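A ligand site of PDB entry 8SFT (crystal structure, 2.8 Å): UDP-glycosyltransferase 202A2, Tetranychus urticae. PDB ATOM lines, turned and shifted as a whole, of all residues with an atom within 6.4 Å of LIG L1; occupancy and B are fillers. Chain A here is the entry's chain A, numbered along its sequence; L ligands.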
ATOM      1  N   LEU A  20      12.920  18.493  25.138  1.00  0.00           N
ATOM      2  CA  LEU A  20      13.491  18.553  23.778  1.00  0.00           C
ATOM      3  C   LEU A  20      12.679  17.615  22.887  1.00  0.00           C
ATOM      4  O   LEU A  20      11.714  17.022  23.388  1.00  0.00           O
ATOM      5  CB  LEU A  20      15.009  18.370  23.755  1.00  0.00           C
ATOM      6  CG  LEU A  20      15.624  17.111  24.345  1.00  0.00           C
ATOM      7  CD1 LEU A  20      15.472  15.923  23.430  1.00  0.00           C
ATOM      8  CD2 LEU A  20      17.096  17.378  24.562  1.00  0.00           C
ATOM      9  N   PHE A  21      12.939  17.657  21.580  1.00  0.00           N
ATOM     10  CA  PHE A  21      12.130  16.979  20.530  1.00  0.00           C
ATOM     11  C   PHE A  21      11.867  15.503  20.861  1.00  0.00           C
ATOM     12  O   PHE A  21      10.776  14.991  20.538  1.00  0.00           O
ATOM     13  CB  PHE A  21      12.827  17.135  19.185  1.00  0.00           C
ATOM     14  CG  PHE A  21      14.135  16.396  19.098  1.00  0.00           C
ATOM     15  CD1 PHE A  21      15.303  16.979  19.568  1.00  0.00           C
ATOM     16  CD2 PHE A  21      14.193  15.114  18.560  1.00  0.00           C
ATOM     17  CE1 PHE A  21      16.497  16.294  19.475  1.00  0.00           C
ATOM     18  CE2 PHE A  21      15.387  14.428  18.481  1.00  0.00           C
ATOM     19  CZ  PHE A  21      16.547  15.022  18.924  1.00  0.00           C
ATOM     20  N   GLY A  22      12.854  14.821  21.439  1.00  0.00           N
ATOM     21  CA  GLY A  22      12.818  13.365  21.693  1.00  0.00           C
ATOM     22  C   GLY A  22      11.544  12.962  22.422  1.00  0.00           C
ATOM     23  O   GLY A  22      11.261  13.461  23.510  1.00  0.00           O
ATOM     24  N   GLY A  24      11.050  10.437  24.188  1.00  0.00           N
ATOM     25  CA  GLY A  24      11.439   9.991  25.543  1.00  0.00           C
ATOM     26  C   GLY A  24      11.293  11.103  26.556  1.00  0.00           C
ATOM     27  O   GLY A  24      10.758  10.853  27.653  1.00  0.00           O
ATOM     28  N   HIS A  25      11.715  12.318  26.205  1.00  0.00           N
ATOM     29  CA  HIS A  25      11.667  13.496  27.097  1.00  0.00           C
ATOM     30  C   HIS A  25      10.213  13.952  27.265  1.00  0.00           C
ATOM     31  O   HIS A  25       9.797  14.217  28.414  1.00  0.00           O
ATOM     32  CB  HIS A  25      12.646  14.549  26.563  1.00  0.00           C
ATOM     33  CG  HIS A  25      14.028  14.017  26.492  1.00  0.00           C
ATOM     34  ND1 HIS A  25      14.928  14.150  27.527  1.00  0.00           N
ATOM     35  CD2 HIS A  25      14.667  13.296  25.534  1.00  0.00           C
ATOM     36  CE1 HIS A  25      16.061  13.576  27.198  1.00  0.00           C
ATOM     37  NE2 HIS A  25      15.927  13.011  25.984  1.00  0.00           N
ATOM     38  N   MET A  78      13.820  18.403  15.095  1.00  0.00           N
ATOM     39  CA  MET A  78      14.926  17.579  14.575  1.00  0.00           C
ATOM     40  C   MET A  78      14.563  16.108  14.528  1.00  0.00           C
ATOM     41  O   MET A  78      15.417  15.313  14.153  1.00  0.00           O
ATOM     42  CB  MET A  78      16.141  17.736  15.487  1.00  0.00           C
ATOM     43  CG  MET A  78      16.687  19.136  15.555  1.00  0.00           C
ATOM     44  SD  MET A  78      18.195  19.183  16.542  1.00  0.00           S
ATOM     45  CE  MET A  78      19.433  19.260  15.239  1.00  0.00           C
ATOM     46  N   ILE A  82      16.899  12.868  12.613  1.00  0.00           N
ATOM     47  CA  ILE A  82      17.837  12.518  13.712  1.00  0.00           C
ATOM     48  C   ILE A  82      18.659  11.292  13.291  1.00  0.00           C
ATOM     49  O   ILE A  82      19.690  11.038  13.921  1.00  0.00           O
ATOM     50  CB  ILE A  82      17.055  12.273  15.014  1.00  0.00           C
ATOM     51  CG1 ILE A  82      17.993  12.071  16.207  1.00  0.00           C
ATOM     52  CG2 ILE A  82      16.088  11.119  14.859  1.00  0.00           C
ATOM     53  CD1 ILE A  82      18.931  13.218  16.449  1.00  0.00           C
ATOM     54  N   ILE A  85      22.454  11.710  12.572  1.00  0.00           N
ATOM     55  CA  ILE A  85      23.235  11.662  13.851  1.00  0.00           C
ATOM     56  C   ILE A  85      23.297  10.209  14.375  1.00  0.00           C
ATOM     57  O   ILE A  85      24.375   9.816  14.840  1.00  0.00           O
ATOM     58  CB  ILE A  85      22.604  12.643  14.865  1.00  0.00           C
ATOM     59  CG1 ILE A  85      22.717  14.081  14.353  1.00  0.00           C
ATOM     60  CG2 ILE A  85      23.186  12.456  16.276  1.00  0.00           C
ATOM     61  CD1 ILE A  85      21.488  14.956  14.578  1.00  0.00           C
ATOM     62  N   HIS A 109      32.343  16.024  23.219  1.00  0.00           N
ATOM     63  CA  HIS A 109      31.286  15.506  24.126  1.00  0.00           C
ATOM     64  C   HIS A 109      30.103  14.992  23.296  1.00  0.00           C
ATOM     65  O   HIS A 109      29.815  15.525  22.206  1.00  0.00           O
ATOM     66  CB  HIS A 109      30.882  16.580  25.143  1.00  0.00           C
ATOM     67  CG  HIS A 109      29.762  16.176  26.046  1.00  0.00           C
ATOM     68  ND1 HIS A 109      28.476  15.977  25.612  1.00  0.00           N
ATOM     69  CD2 HIS A 109      29.740  15.958  27.367  1.00  0.00           C
ATOM     70  CE1 HIS A 109      27.714  15.636  26.629  1.00  0.00           C
ATOM     71  NE2 HIS A 109      28.453  15.618  27.713  1.00  0.00           N
ATOM     72  N   THR A 110      29.461  13.947  23.818  1.00  0.00           N
ATOM     73  CA  THR A 110      28.304  13.246  23.181  1.00  0.00           C
ATOM     74  C   THR A 110      27.271  14.242  22.629  1.00  0.00           C
ATOM     75  O   THR A 110      26.835  14.018  21.500  1.00  0.00           O
ATOM     76  CB  THR A 110      27.678  12.249  24.159  1.00  0.00           C
ATOM     77  OG1 THR A 110      28.747  11.449  24.654  1.00  0.00           O
ATOM     78  CG2 THR A 110      26.589  11.389  23.546  1.00  0.00           C
ATOM     79  N   PHE A 111      26.903  15.301  23.360  1.00  0.00           N
ATOM     80  CA  PHE A 111      25.810  16.224  22.947  1.00  0.00           C
ATOM     81  C   PHE A 111      26.187  17.706  23.082  1.00  0.00           C
ATOM     82  O   PHE A 111      25.290  18.543  22.948  1.00  0.00           O
ATOM     83  CB  PHE A 111      24.512  15.871  23.680  1.00  0.00           C
ATOM     84  CG  PHE A 111      24.558  15.858  25.190  1.00  0.00           C
ATOM     85  CD1 PHE A 111      24.645  17.050  25.899  1.00  0.00           C
ATOM     86  CD2 PHE A 111      24.430  14.669  25.895  1.00  0.00           C
ATOM     87  CE1 PHE A 111      24.655  17.041  27.288  1.00  0.00           C
ATOM     88  CE2 PHE A 111      24.421  14.669  27.279  1.00  0.00           C
ATOM     89  CZ  PHE A 111      24.559  15.846  27.976  1.00  0.00           C
ATOM     90  N   ALA A 112      27.458  18.071  23.210  1.00  0.00           N
ATOM     91  CA  ALA A 112      27.924  19.484  23.155  1.00  0.00           C
ATOM     92  C   ALA A 112      27.562  20.162  21.808  1.00  0.00           C
ATOM     93  O   ALA A 112      27.317  21.398  21.819  1.00  0.00           O
ATOM     94  CB  ALA A 112      29.399  19.570  23.423  1.00  0.00           C
ATOM     95  N   GLY A 113      27.505  19.397  20.697  1.00  0.00           N
ATOM     96  CA  GLY A 113      27.113  19.927  19.366  1.00  0.00           C
ATOM     97  C   GLY A 113      25.705  20.522  19.306  1.00  0.00           C
ATOM     98  O   GLY A 113      25.428  21.372  18.436  1.00  0.00           O
ATOM     99  N   MET A 114      24.784  20.080  20.166  1.00  0.00           N
ATOM    100  CA  MET A 114      23.392  20.599  20.249  1.00  0.00           C
ATOM    101  C   MET A 114      23.350  21.982  20.893  1.00  0.00           C
ATOM    102  O   MET A 114      22.341  22.674  20.749  1.00  0.00           O
ATOM    103  CB  MET A 114      22.540  19.725  21.166  1.00  0.00           C
ATOM    104  CG  MET A 114      22.330  18.321  20.745  1.00  0.00           C
ATOM    105  SD  MET A 114      21.034  17.681  21.840  1.00  0.00           S
ATOM    106  CE  MET A 114      19.644  18.700  21.335  1.00  0.00           C
ATOM    107  N   LEU A 142      18.552  17.915  28.053  1.00  0.00           N
ATOM    108  CA  LEU A 142      19.829  17.218  28.350  1.00  0.00           C
ATOM    109  C   LEU A 142      20.729  18.114  29.194  1.00  0.00           C
ATOM    110  O   LEU A 142      21.704  17.578  29.758  1.00  0.00           O
ATOM    111  CB  LEU A 142      20.530  16.839  27.053  1.00  0.00           C
ATOM    112  CG  LEU A 142      19.881  15.715  26.241  1.00  0.00           C
ATOM    113  CD1 LEU A 142      20.656  15.493  24.971  1.00  0.00           C
ATOM    114  CD2 LEU A 142      19.787  14.407  27.023  1.00  0.00           C
ATOM    115  N   SER A 160      15.073  12.341  32.671  1.00  0.00           N
ATOM    116  CA  SER A 160      14.525  11.034  32.274  1.00  0.00           C
ATOM    117  C   SER A 160      15.673  10.131  31.830  1.00  0.00           C
ATOM    118  O   SER A 160      15.477   8.907  31.825  1.00  0.00           O
ATOM    119  CB  SER A 160      13.485  11.191  31.221  1.00  0.00           C
ATOM    120  OG  SER A 160      13.997  11.835  30.057  1.00  0.00           O
ATOM    121  N   VAL A 161      16.850  10.700  31.555  1.00  0.00           N
ATOM    122  CA  VAL A 161      18.069   9.894  31.250  1.00  0.00           C
ATOM    123  C   VAL A 161      18.577   9.257  32.548  1.00  0.00           C
ATOM    124  O   VAL A 161      18.159   9.674  33.647  1.00  0.00           O
ATOM    125  CB  VAL A 161      19.171  10.736  30.576  1.00  0.00           C
ATOM    126  CG1 VAL A 161      18.705  11.401  29.289  1.00  0.00           C
ATOM    127  CG2 VAL A 161      19.718  11.787  31.514  1.00  0.00           C
ATOM    128  N   LEU A 280      14.611   7.229  18.310  1.00  0.00           N
ATOM    129  CA  LEU A 280      15.710   7.960  17.629  1.00  0.00           C
ATOM    130  C   LEU A 280      16.549   6.970  16.821  1.00  0.00           C
ATOM    131  O   LEU A 280      16.608   7.133  15.581  1.00  0.00           O
ATOM    132  CB  LEU A 280      16.549   8.686  18.687  1.00  0.00           C
ATOM    133  CG  LEU A 280      15.768   9.578  19.662  1.00  0.00           C
ATOM    134  CD1 LEU A 280      16.698  10.222  20.665  1.00  0.00           C
ATOM    135  CD2 LEU A 280      14.952  10.638  18.926  1.00  0.00           C
ATOM    136  N   PHE A 362      23.925   5.134  21.989  1.00  0.00           N
ATOM    137  CA  PHE A 362      24.619   6.403  22.351  1.00  0.00           C
ATOM    138  C   PHE A 362      24.175   6.874  23.735  1.00  0.00           C
ATOM    139  O   PHE A 362      23.025   6.633  24.138  1.00  0.00           O
ATOM    140  CB  PHE A 362      24.352   7.468  21.277  1.00  0.00           C
ATOM    141  CG  PHE A 362      22.909   7.815  21.041  1.00  0.00           C
ATOM    142  CD1 PHE A 362      22.227   8.644  21.920  1.00  0.00           C
ATOM    143  CD2 PHE A 362      22.225   7.309  19.954  1.00  0.00           C
ATOM    144  CE1 PHE A 362      20.893   8.961  21.696  1.00  0.00           C
ATOM    145  CE2 PHE A 362      20.900   7.635  19.731  1.00  0.00           C
ATOM    146  CZ  PHE A 362      20.238   8.458  20.601  1.00  0.00           C
ATOM    147  N   GLY A 363      25.090   7.538  24.454  1.00  0.00           N
ATOM    148  CA  GLY A 363      24.767   8.375  25.616  1.00  0.00           C
ATOM    149  C   GLY A 363      24.439   7.556  26.855  1.00  0.00           C
ATOM    150  O   GLY A 363      25.219   6.657  27.198  1.00  0.00           O
ATOM    151  N   ASP A 364      23.324   7.902  27.507  1.00  0.00           N
ATOM    152  CA  ASP A 364      22.902   7.274  28.786  1.00  0.00           C
ATOM    153  C   ASP A 364      22.532   5.817  28.519  1.00  0.00           C
ATOM    154  O   ASP A 364      22.512   5.035  29.478  1.00  0.00           O
ATOM    155  CB  ASP A 364      21.736   8.051  29.407  1.00  0.00           C
ATOM    156  CG  ASP A 364      20.456   7.962  28.605  1.00  0.00           C
ATOM    157  OD1 ASP A 364      20.475   8.360  27.427  1.00  0.00           O
ATOM    158  OD2 ASP A 364      19.434   7.506  29.163  1.00  0.00           O
ATOM    159  N   GLN A 365      22.246   5.489  27.256  1.00  0.00           N
ATOM    160  CA  GLN A 365      21.905   4.083  26.919  1.00  0.00           C
ATOM    161  C   GLN A 365      23.021   3.138  27.405  1.00  0.00           C
ATOM    162  O   GLN A 365      22.652   2.046  27.893  1.00  0.00           O
ATOM    163  CB  GLN A 365      21.663   3.924  25.427  1.00  0.00           C
ATOM    164  CG  GLN A 365      20.483   4.741  24.904  1.00  0.00           C
ATOM    165  CD  GLN A 365      20.596   4.932  23.423  1.00  0.00           C
ATOM    166  OE1 GLN A 365      21.254   4.171  22.731  1.00  0.00           O
ATOM    167  NE2 GLN A 365      19.959   5.957  22.926  1.00  0.00           N
HETATM  168  C1  LIG L   1      22.198  16.025  17.928  1.00  0.00           C
HETATM  169  C2  LIG L   1      22.947  15.262  18.789  1.00  0.00           C
HETATM  170  C3  LIG L   1      22.326  14.510  19.807  1.00  0.00           C
HETATM  171  C4  LIG L   1      20.934  14.589  19.906  1.00  0.00           C
HETATM  172  C5  LIG L   1      20.149  15.351  19.068  1.00  0.00           C
HETATM  173  C6  LIG L   1      20.802  16.072  18.072  1.00  0.00           C
HETATM  174  C7  LIG L   1      23.061  13.680  20.749  1.00  0.00           C
HETATM  175  C8  LIG L   1      22.273  12.976  21.732  1.00  0.00           C
HETATM  176  C9  LIG L   1      20.919  13.097  21.773  1.00  0.00           C
HETATM  177  C10 LIG L   1      20.028  12.431  22.740  1.00  0.00           C
HETATM  178  C11 LIG L   1      20.540  11.684  23.807  1.00  0.00           C
HETATM  179  C12 LIG L   1      19.705  11.082  24.719  1.00  0.00           C
HETATM  180  C13 LIG L   1      18.328  11.203  24.581  1.00  0.00           C
HETATM  181  C14 LIG L   1      17.805  11.948  23.534  1.00  0.00           C
HETATM  182  C15 LIG L   1      18.645  12.554  22.631  1.00  0.00           C
HETATM  183  O1  LIG L   1      20.270  13.893  20.872  1.00  0.00           O
HETATM  184  O2  LIG L   1      24.308  13.556  20.726  1.00  0.00           O
HETATM  185  O3  LIG L   1      17.493  10.601  25.492  1.00  0.00           O
HETATM  186  O4  LIG L   1      22.956  12.191  22.620  1.00  0.00           O
HETATM  187  O5  LIG L   1      20.062  16.846  17.213  1.00  0.00           O
HETATM  188  O6  LIG L   1      24.306  15.196  18.679  1.00  0.00           O
HETATM  189  N1  LG2 L   2       7.687   4.211  22.095  1.00  0.00           N
HETATM  190  C1  LG2 L   2       6.372   3.861  21.820  1.00  0.00           C
HETATM  191  N2  LG2 L   2       6.210   3.065  20.714  1.00  0.00           N
HETATM  192  C2  LG2 L   2       7.204   2.589  19.884  1.00  0.00           C
HETATM  193  C3  LG2 L   2       8.525   2.989  20.233  1.00  0.00           C
HETATM  194  C4  LG2 L   2       8.721   3.769  21.313  1.00  0.00           C
HETATM  195  O1  LG2 L   2       5.426   4.242  22.501  1.00  0.00           O
HETATM  196  O2  LG2 L   2       6.886   1.870  18.929  1.00  0.00           O
HETATM  197  C5  LG2 L   2       7.913   5.063  23.274  1.00  0.00           C
HETATM  198  C6  LG2 L   2       8.221   4.265  24.535  1.00  0.00           C
HETATM  199  O3  LG2 L   2       6.996   3.886  25.145  1.00  0.00           O
HETATM  200  C7  LG2 L   2       9.013   5.289  25.357  1.00  0.00           C
HETATM  201  C8  LG2 L   2       9.747   6.120  24.292  1.00  0.00           C
HETATM  202  O4  LG2 L   2       9.052   5.859  23.037  1.00  0.00           O
HETATM  203  O5  LG2 L   2       8.154   6.120  26.143  1.00  0.00           O
HETATM  204  C9  LG2 L   2      11.211   5.815  24.132  1.00  0.00           C
HETATM  205  O6  LG2 L   2      11.935   6.376  25.257  1.00  0.00           O
HETATM  206  P1  LG2 L   2      13.395   5.806  25.593  1.00  0.00           P
HETATM  207  O7  LG2 L   2      13.287   4.351  25.943  1.00  0.00           O
HETATM  208  O8  LG2 L   2      14.069   6.702  26.568  1.00  0.00           O
HETATM  209  O9  LG2 L   2      14.117   5.933  24.169  1.00  0.00           O
HETATM  210  P2  LG2 L   2      14.791   7.147  23.361  1.00  0.00           P
HETATM  211  O10 LG2 L   2      14.946   6.671  21.944  1.00  0.00           O
HETATM  212  O11 LG2 L   2      16.113   7.409  24.036  1.00  0.00           O
HETATM  213  O12 LG2 L   2      13.843   8.314  23.480  1.00  0.00           O
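O of Thr 110 lies close to O2 of LIG L1 (2.7 Å).
NE2 of His 25 lies within hydrogen-bond range of O3 of LIG L1, 2.9 Å away.
The side-chain sulfur (SD) of Met 78 sits at hydrogen-bond distance from an oxygen (O5) of LIG L1.
Residues that only touch LIG L1: Phe 362, Leu 280, Ile 85, Ile 82, Phe 21, Met 114, Phe 111, Leu 142 and Asp 364.
12 residues have an atom within 4 Å of LIG L1: Phe 21, His 25, Met 78, Ile 82, Ile 85, Thr 110, Phe 111, Met 114, Leu 142, Leu 280, Phe 362 and Asp 364.
N of Phe 362 sits at hydrogen-bond distance from OE1 of Gln 365 (2.9 Å).
The backbone NH (N) of Phe 111 lies within hydrogen-bond range of a ring nitrogen (ND1) of His 109 (2.8 Å).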
